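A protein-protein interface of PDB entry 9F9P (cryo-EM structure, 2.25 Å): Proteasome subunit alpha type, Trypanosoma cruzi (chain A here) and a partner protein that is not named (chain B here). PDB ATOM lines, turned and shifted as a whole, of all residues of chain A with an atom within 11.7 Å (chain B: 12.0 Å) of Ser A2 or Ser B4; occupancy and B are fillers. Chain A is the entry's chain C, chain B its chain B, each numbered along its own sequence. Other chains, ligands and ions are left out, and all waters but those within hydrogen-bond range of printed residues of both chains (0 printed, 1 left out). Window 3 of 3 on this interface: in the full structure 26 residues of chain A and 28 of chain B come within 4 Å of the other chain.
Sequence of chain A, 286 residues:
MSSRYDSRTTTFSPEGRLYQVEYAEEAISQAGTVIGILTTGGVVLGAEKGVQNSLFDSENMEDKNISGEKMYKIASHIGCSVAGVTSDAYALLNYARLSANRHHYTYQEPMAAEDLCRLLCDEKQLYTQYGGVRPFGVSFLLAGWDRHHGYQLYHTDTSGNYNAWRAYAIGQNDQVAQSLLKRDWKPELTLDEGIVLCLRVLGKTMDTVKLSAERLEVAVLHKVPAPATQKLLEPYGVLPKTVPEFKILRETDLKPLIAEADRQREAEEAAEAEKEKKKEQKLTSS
Of the 10 printed residues of chain A, 5 touch a printed residue of chain B.
Of the 14 printed residues of chain B, 6 touch a printed residue of chain A.
The backbone carbonyl oxygen (O) of Glu B118 lies close to the side-chain hydroxyl (OG) of Ser B122, 3.5 Å away.
The side-chain carboxylate (OD1) of Asp A6 sits at hydrogen-bond distance from the backbone NH (N) of Arg A8.
The backbone carbonyl oxygen of Tyr B6 lies within hydrogen-bond range of the backbone NH of Gly B124 (2.7 Å).
The backbone NH (N) of Gly B7 sits at hydrogen-bond distance from the backbone carbonyl oxygen (O) of Gly A132, 3.0 Å away.
The backbone carbonyl oxygen (O) of Ser A2 lies close to the side-chain hydroxyl (OH) of Tyr B6 (2.3 Å).
OG of Ser B4 is in hydrogen-bond range of OG of Ser A2 (2.8 Å).
Among the printed residues, pairs that only touch across the chains: Tyr A5 with Tyr B6, Asp A6 with Tyr B6, Gly A132 with Tyr B6, Val A133 with Gln B121, Val A133 with Ser B122 and Val A133 with Gly B123.
Ser A2 touches two residues of chain B.
Of chain A, only Ser A2 (2.8 Å) comes within 4 Å of Ser B4.
Ser A3 touches none of the printed residues of chain B.
Of chain B, only Tyr B6 (3.4 Å) comes within 4 Å of Tyr A5.
Of chain B, only Tyr B6 comes within 4 Å of Asp A6.
Of chain A, only Val A133 (3.8 Å) comes within 4 Å of Gly B123.
Gly B124 touches none of the printed residues of chain A.
Of the printed residues of chain A, Ser B122 touches Val A133 (3.997 Å).
Printed residues of chain B within 4 Å of Gly A132: Tyr B6 (3.6 Å) and Gly B7 (3.0 Å).
Of the printed residues of chain B, Val A133 touches Gln B121 (3.3 Å), Ser B122 (3.997 Å) and Gly B123 (3.8 Å).
Of the printed residues of chain A, Gly B7 touches Gly A132.
Printed residues of chain A within 4 Å of Gln B121: Val A133 (3.3 Å).
Gly A131 touches none of the printed residues of chain B.
Arg B126 touches none of the printed residues of chain A.
The nearest residue of chain B that does not touch Ser A2 is Ala B5 (6.9 Å).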
ATOM      1  N   SER A   2       0.525 -11.951 -14.485  1.00  0.00           N
ATOM      2  CA  SER A   2       0.926 -10.636 -13.919  1.00  0.00           C
ATOM      3  C   SER A   2      -0.336  -9.861 -13.546  1.00  0.00           C
ATOM      4  O   SER A   2      -0.280  -9.132 -12.555  1.00  0.00           O
ATOM      5  CB  SER A   2       1.856  -9.788 -14.808  1.00  0.00           C
ATOM      6  OG  SER A   2       3.082  -9.423 -14.150  1.00  0.00           O
ATOM      7  N   SER A   3      -1.465 -10.046 -14.260  1.00  0.00           N
ATOM      8  CA  SER A   3      -2.687  -9.325 -13.908  1.00  0.00           C
ATOM      9  C   SER A   3      -3.280  -9.770 -12.569  1.00  0.00           C
ATOM     10  O   SER A   3      -3.999  -9.003 -11.957  1.00  0.00           O
ATOM     11  CB  SER A   3      -3.755  -9.368 -14.982  1.00  0.00           C
ATOM     12  OG  SER A   3      -4.683 -10.421 -14.742  1.00  0.00           O
ATOM     13  N   ARG A   4      -2.961 -10.954 -12.062  1.00  0.00           N
ATOM     14  CA  ARG A   4      -3.495 -11.352 -10.770  1.00  0.00           C
ATOM     15  C   ARG A   4      -2.803 -10.652  -9.598  1.00  0.00           C
ATOM     16  O   ARG A   4      -3.273 -10.770  -8.474  1.00  0.00           O
ATOM     17  CB  ARG A   4      -3.441 -12.873 -10.581  1.00  0.00           C
ATOM     18  CG  ARG A   4      -2.103 -13.523 -10.865  1.00  0.00           C
ATOM     19  CD  ARG A   4      -2.229 -15.013 -11.155  1.00  0.00           C
ATOM     20  NE  ARG A   4      -2.447 -15.774  -9.932  1.00  0.00           N
ATOM     21  CZ  ARG A   4      -3.329 -16.760  -9.789  1.00  0.00           C
ATOM     22  NH1 ARG A   4      -3.491 -17.323  -8.604  1.00  0.00           N
ATOM     23  NH2 ARG A   4      -4.052 -17.174 -10.822  1.00  0.00           N
ATOM     24  N   TYR A   5      -1.678  -9.964  -9.842  1.00  0.00           N
ATOM     25  CA  TYR A   5      -0.986  -9.216  -8.798  1.00  0.00           C
ATOM     26  C   TYR A   5      -1.230  -7.708  -8.937  1.00  0.00           C
ATOM     27  O   TYR A   5      -0.561  -6.937  -8.260  1.00  0.00           O
ATOM     28  CB  TYR A   5       0.525  -9.531  -8.803  1.00  0.00           C
ATOM     29  CG  TYR A   5       0.859 -11.009  -8.799  1.00  0.00           C
ATOM     30  CD1 TYR A   5       0.509 -11.823  -7.729  1.00  0.00           C
ATOM     31  CD2 TYR A   5       1.415 -11.626  -9.918  1.00  0.00           C
ATOM     32  CE1 TYR A   5       0.756 -13.193  -7.746  1.00  0.00           C
ATOM     33  CE2 TYR A   5       1.644 -12.995  -9.960  1.00  0.00           C
ATOM     34  CZ  TYR A   5       1.311 -13.785  -8.873  1.00  0.00           C
ATOM     35  OH  TYR A   5       1.563 -15.141  -8.919  1.00  0.00           O
ATOM     36  N   ASP A   6      -2.179  -7.276  -9.786  1.00  0.00           N
ATOM     37  CA  ASP A   6      -2.522  -5.861  -9.914  1.00  0.00           C
ATOM     38  C   ASP A   6      -3.395  -5.472  -8.724  1.00  0.00           C
ATOM     39  O   ASP A   6      -4.336  -6.181  -8.415  1.00  0.00           O
ATOM     40  CB  ASP A   6      -3.185  -5.579 -11.276  1.00  0.00           C
ATOM     41  CG  ASP A   6      -3.681  -4.166 -11.600  1.00  0.00           C
ATOM     42  OD1 ASP A   6      -3.645  -3.302 -10.719  1.00  0.00           O
ATOM     43  OD2 ASP A   6      -4.139  -3.945 -12.756  1.00  0.00           O
ATOM     44  N   SER A   7      -3.066  -4.360  -8.055  1.00  0.00           N
ATOM     45  CA  SER A   7      -3.801  -3.944  -6.861  1.00  0.00           C
ATOM     46  C   SER A   7      -4.995  -3.023  -7.158  1.00  0.00           C
ATOM     47  O   SER A   7      -5.758  -2.743  -6.251  1.00  0.00           O
ATOM     48  CB  SER A   7      -2.854  -3.301  -5.873  1.00  0.00           C
ATOM     49  OG  SER A   7      -2.365  -2.070  -6.398  1.00  0.00           O
ATOM     50  N   ARG A   8      -5.153  -2.541  -8.405  1.00  0.00           N
ATOM     51  CA  ARG A   8      -6.352  -1.843  -8.878  1.00  0.00           C
ATOM     52  C   ARG A   8      -6.544  -0.529  -8.105  1.00  0.00           C
ATOM     53  O   ARG A   8      -7.470  -0.375  -7.317  1.00  0.00           O
ATOM     54  CB  ARG A   8      -7.571  -2.779  -8.815  1.00  0.00           C
ATOM     55  CG  ARG A   8      -7.393  -4.100  -9.564  1.00  0.00           C
ATOM     56  CD  ARG A   8      -8.644  -4.806 -10.070  1.00  0.00           C
ATOM     57  NE  ARG A   8      -8.340  -6.004 -10.868  1.00  0.00           N
ATOM     58  CZ  ARG A   8      -8.380  -6.085 -12.209  1.00  0.00           C
ATOM     59  NH1 ARG A   8      -7.931  -7.174 -12.820  1.00  0.00           N
ATOM     60  NH2 ARG A   8      -8.813  -5.066 -12.939  1.00  0.00           N
ATOM     61  N   GLY A 131      -4.467   5.289 -15.197  1.00  0.00           N
ATOM     62  CA  GLY A 131      -3.062   4.912 -15.289  1.00  0.00           C
ATOM     63  C   GLY A 131      -2.515   3.940 -14.236  1.00  0.00           C
ATOM     64  O   GLY A 131      -1.308   3.675 -14.239  1.00  0.00           O
ATOM     65  N   GLY A 132      -3.326   3.346 -13.379  1.00  0.00           N
ATOM     66  CA  GLY A 132      -2.798   2.205 -12.621  1.00  0.00           C
ATOM     67  C   GLY A 132      -1.673   2.392 -11.576  1.00  0.00           C
ATOM     68  O   GLY A 132      -1.179   1.388 -11.092  1.00  0.00           O
ATOM     69  N   VAL A 133      -1.331   3.606 -11.101  1.00  0.00           N
ATOM     70  CA  VAL A 133      -0.325   3.797 -10.042  1.00  0.00           C
ATOM     71  C   VAL A 133      -0.884   4.519  -8.813  1.00  0.00           C
ATOM     72  O   VAL A 133      -1.981   5.023  -8.821  1.00  0.00           O
ATOM     73  CB  VAL A 133       0.906   4.528 -10.605  1.00  0.00           C
ATOM     74  CG1 VAL A 133       1.521   3.778 -11.775  1.00  0.00           C
ATOM     75  CG2 VAL A 133       0.627   5.954 -11.048  1.00  0.00           C
ATOM     76  N   SER B   4       4.328  -5.269 -18.010  1.00  0.00           N
ATOM     77  CA  SER B   4       3.541  -4.933 -16.785  1.00  0.00           C
ATOM     78  C   SER B   4       3.631  -3.430 -16.486  1.00  0.00           C
ATOM     79  O   SER B   4       4.701  -2.819 -16.523  1.00  0.00           O
ATOM     80  CB  SER B   4       3.932  -5.769 -15.573  1.00  0.00           C
ATOM     81  OG  SER B   4       3.170  -6.975 -15.495  1.00  0.00           O
ATOM     82  N   ALA B   5       2.471  -2.834 -16.206  1.00  0.00           N
ATOM     83  CA  ALA B   5       2.372  -1.398 -16.178  1.00  0.00           C
ATOM     84  C   ALA B   5       1.507  -0.919 -15.010  1.00  0.00           C
ATOM     85  O   ALA B   5       1.012   0.189 -15.055  1.00  0.00           O
ATOM     86  CB  ALA B   5       1.796  -1.000 -17.501  1.00  0.00           C
ATOM     87  N   TYR B   6       1.321  -1.722 -13.971  1.00  0.00           N
ATOM     88  CA  TYR B   6       0.667  -1.266 -12.766  1.00  0.00           C
ATOM     89  C   TYR B   6       1.686  -1.029 -11.646  1.00  0.00           C
ATOM     90  O   TYR B   6       2.799  -1.515 -11.676  1.00  0.00           O
ATOM     91  CB  TYR B   6      -0.414  -2.255 -12.325  1.00  0.00           C
ATOM     92  CG  TYR B   6       0.033  -3.687 -12.132  1.00  0.00           C
ATOM     93  CD1 TYR B   6       0.660  -4.115 -10.965  1.00  0.00           C
ATOM     94  CD2 TYR B   6      -0.175  -4.629 -13.133  1.00  0.00           C
ATOM     95  CE1 TYR B   6       1.115  -5.433 -10.811  1.00  0.00           C
ATOM     96  CE2 TYR B   6       0.219  -5.954 -12.980  1.00  0.00           C
ATOM     97  CZ  TYR B   6       0.899  -6.353 -11.834  1.00  0.00           C
ATOM     98  OH  TYR B   6       1.263  -7.665 -11.731  1.00  0.00           O
ATOM     99  N   GLY B   7       1.272  -0.301 -10.617  1.00  0.00           N
ATOM    100  CA  GLY B   7       2.172   0.072  -9.554  1.00  0.00           C
ATOM    101  C   GLY B   7       2.366  -1.052  -8.544  1.00  0.00           C
ATOM    102  O   GLY B   7       1.411  -1.755  -8.171  1.00  0.00           O
ATOM    103  N   LEU B   8       3.599  -1.135  -8.040  1.00  0.00           N
ATOM    104  CA  LEU B   8       3.971  -2.161  -7.086  1.00  0.00           C
ATOM    105  C   LEU B   8       4.053  -1.576  -5.681  1.00  0.00           C
ATOM    106  O   LEU B   8       3.986  -2.332  -4.727  1.00  0.00           O
ATOM    107  CB  LEU B   8       5.311  -2.751  -7.525  1.00  0.00           C
ATOM    108  CG  LEU B   8       5.302  -3.441  -8.892  1.00  0.00           C
ATOM    109  CD1 LEU B   8       6.674  -4.001  -9.213  1.00  0.00           C
ATOM    110  CD2 LEU B   8       4.248  -4.544  -8.947  1.00  0.00           C
ATOM    111  N   THR B   9       4.180  -0.251  -5.585  1.00  0.00           N
ATOM    112  CA  THR B   9       4.227   0.473  -4.317  1.00  0.00           C
ATOM    113  C   THR B   9       2.883   1.169  -4.101  1.00  0.00           C
ATOM    114  O   THR B   9       2.503   1.957  -4.963  1.00  0.00           O
ATOM    115  CB  THR B   9       5.349   1.537  -4.346  1.00  0.00           C
ATOM    116  OG1 THR B   9       6.618   0.996  -4.729  1.00  0.00           O
ATOM    117  CG2 THR B   9       5.502   2.260  -3.026  1.00  0.00           C
ATOM    118  N   GLU B 118      10.854   8.459  -8.781  1.00  0.00           N
ATOM    119  CA  GLU B 118      10.163   7.768  -9.870  1.00  0.00           C
ATOM    120  C   GLU B 118      10.000   6.266  -9.641  1.00  0.00           C
ATOM    121  O   GLU B 118       8.995   5.723 -10.026  1.00  0.00           O
ATOM    122  CB  GLU B 118      10.891   7.861 -11.206  1.00  0.00           C
ATOM    123  CG  GLU B 118      10.794   9.207 -11.881  1.00  0.00           C
ATOM    124  CD  GLU B 118      11.793   9.364 -13.032  1.00  0.00           C
ATOM    125  OE1 GLU B 118      11.879   8.425 -13.876  1.00  0.00           O
ATOM    126  OE2 GLU B 118      12.512  10.416 -13.080  1.00  0.00           O
ATOM    127  N   PHE B 119      10.988   5.581  -9.075  1.00  0.00           N
ATOM    128  CA  PHE B 119      10.883   4.152  -8.795  1.00  0.00           C
ATOM    129  C   PHE B 119      10.000   3.858  -7.569  1.00  0.00           C
ATOM    130  O   PHE B 119       9.732   2.690  -7.301  1.00  0.00           O
ATOM    131  CB  PHE B 119      12.272   3.506  -8.720  1.00  0.00           C
ATOM    132  CG  PHE B 119      12.905   3.296 -10.078  1.00  0.00           C
ATOM    133  CD1 PHE B 119      12.983   2.030 -10.653  1.00  0.00           C
ATOM    134  CD2 PHE B 119      13.417   4.370 -10.810  1.00  0.00           C
ATOM    135  CE1 PHE B 119      13.497   1.855 -11.937  1.00  0.00           C
ATOM    136  CE2 PHE B 119      13.949   4.193 -12.086  1.00  0.00           C
ATOM    137  CZ  PHE B 119      13.993   2.932 -12.651  1.00  0.00           C
ATOM    138  N   GLN B 121       6.822   5.202  -7.640  1.00  0.00           N
ATOM    139  CA  GLN B 121       5.508   5.541  -8.152  1.00  0.00           C
ATOM    140  C   GLN B 121       5.203   4.929  -9.531  1.00  0.00           C
ATOM    141  O   GLN B 121       4.100   4.442  -9.742  1.00  0.00           O
ATOM    142  CB  GLN B 121       5.367   7.054  -8.248  1.00  0.00           C
ATOM    143  CG  GLN B 121       3.925   7.490  -8.447  1.00  0.00           C
ATOM    144  CD  GLN B 121       3.700   8.975  -8.347  1.00  0.00           C
ATOM    145  OE1 GLN B 121       4.613   9.776  -8.529  1.00  0.00           O
ATOM    146  NE2 GLN B 121       2.462   9.359  -8.058  1.00  0.00           N
ATOM    147  N   SER B 122       6.144   4.884 -10.460  1.00  0.00           N
ATOM    148  CA  SER B 122       5.912   4.352 -11.799  1.00  0.00           C
ATOM    149  C   SER B 122       5.424   2.916 -11.787  1.00  0.00           C
ATOM    150  O   SER B 122       5.587   2.178 -10.818  1.00  0.00           O
ATOM    151  CB  SER B 122       7.198   4.441 -12.634  1.00  0.00           C
ATOM    152  OG  SER B 122       7.385   5.781 -13.087  1.00  0.00           O
ATOM    153  N   GLY B 123       4.935   2.493 -12.944  1.00  0.00           N
ATOM    154  CA  GLY B 123       4.364   1.169 -13.091  1.00  0.00           C
ATOM    155  C   GLY B 123       5.412   0.105 -13.369  1.00  0.00           C
ATOM    156  O   GLY B 123       6.350   0.321 -14.120  1.00  0.00           O
ATOM    157  N   GLY B 124       5.248  -1.049 -12.744  1.00  0.00           N
ATOM    158  CA  GLY B 124       6.105  -2.177 -13.057  1.00  0.00           C
ATOM    159  C   GLY B 124       7.496  -2.211 -12.405  1.00  0.00           C
ATOM    160  O   GLY B 124       8.281  -3.034 -12.829  1.00  0.00           O
ATOM    161  N   VAL B 125       7.797  -1.379 -11.392  1.00  0.00           N
ATOM    162  CA  VAL B 125       9.131  -1.289 -10.811  1.00  0.00           C
ATOM    163  C   VAL B 125       9.077  -1.235  -9.297  1.00  0.00           C
ATOM    164  O   VAL B 125       8.189  -0.614  -8.757  1.00  0.00           O
ATOM    165  CB  VAL B 125       9.897  -0.050 -11.330  1.00  0.00           C
ATOM    166  CG1 VAL B 125      10.127  -0.075 -12.829  1.00  0.00           C
ATOM    167  CG2 VAL B 125       9.205   1.250 -11.005  1.00  0.00           C
ATOM    168  N   ARG B 126      10.102  -1.759  -8.635  1.00  0.00           N
ATOM    169  CA  ARG B 126      10.251  -1.637  -7.198  1.00  0.00           C
ATOM    170  C   ARG B 126      11.261  -0.532  -6.886  1.00  0.00           C
ATOM    171  O   ARG B 126      12.070  -0.144  -7.724  1.00  0.00           O
ATOM    172  CB  ARG B 126      10.763  -2.946  -6.580  1.00  0.00           C
ATOM    173  CG  ARG B 126      12.154  -3.363  -7.072  1.00  0.00           C
ATOM    174  CD  ARG B 126      12.927  -4.301  -6.183  1.00  0.00           C
ATOM    175  NE  ARG B 126      14.186  -4.747  -6.782  1.00  0.00           N
ATOM    176  CZ  ARG B 126      15.320  -4.059  -6.775  1.00  0.00           C
ATOM    177  NH1 ARG B 126      16.349  -4.486  -7.465  1.00  0.00           N
ATOM    178  NH2 ARG B 126      15.439  -2.920  -6.124  1.00  0.00           N
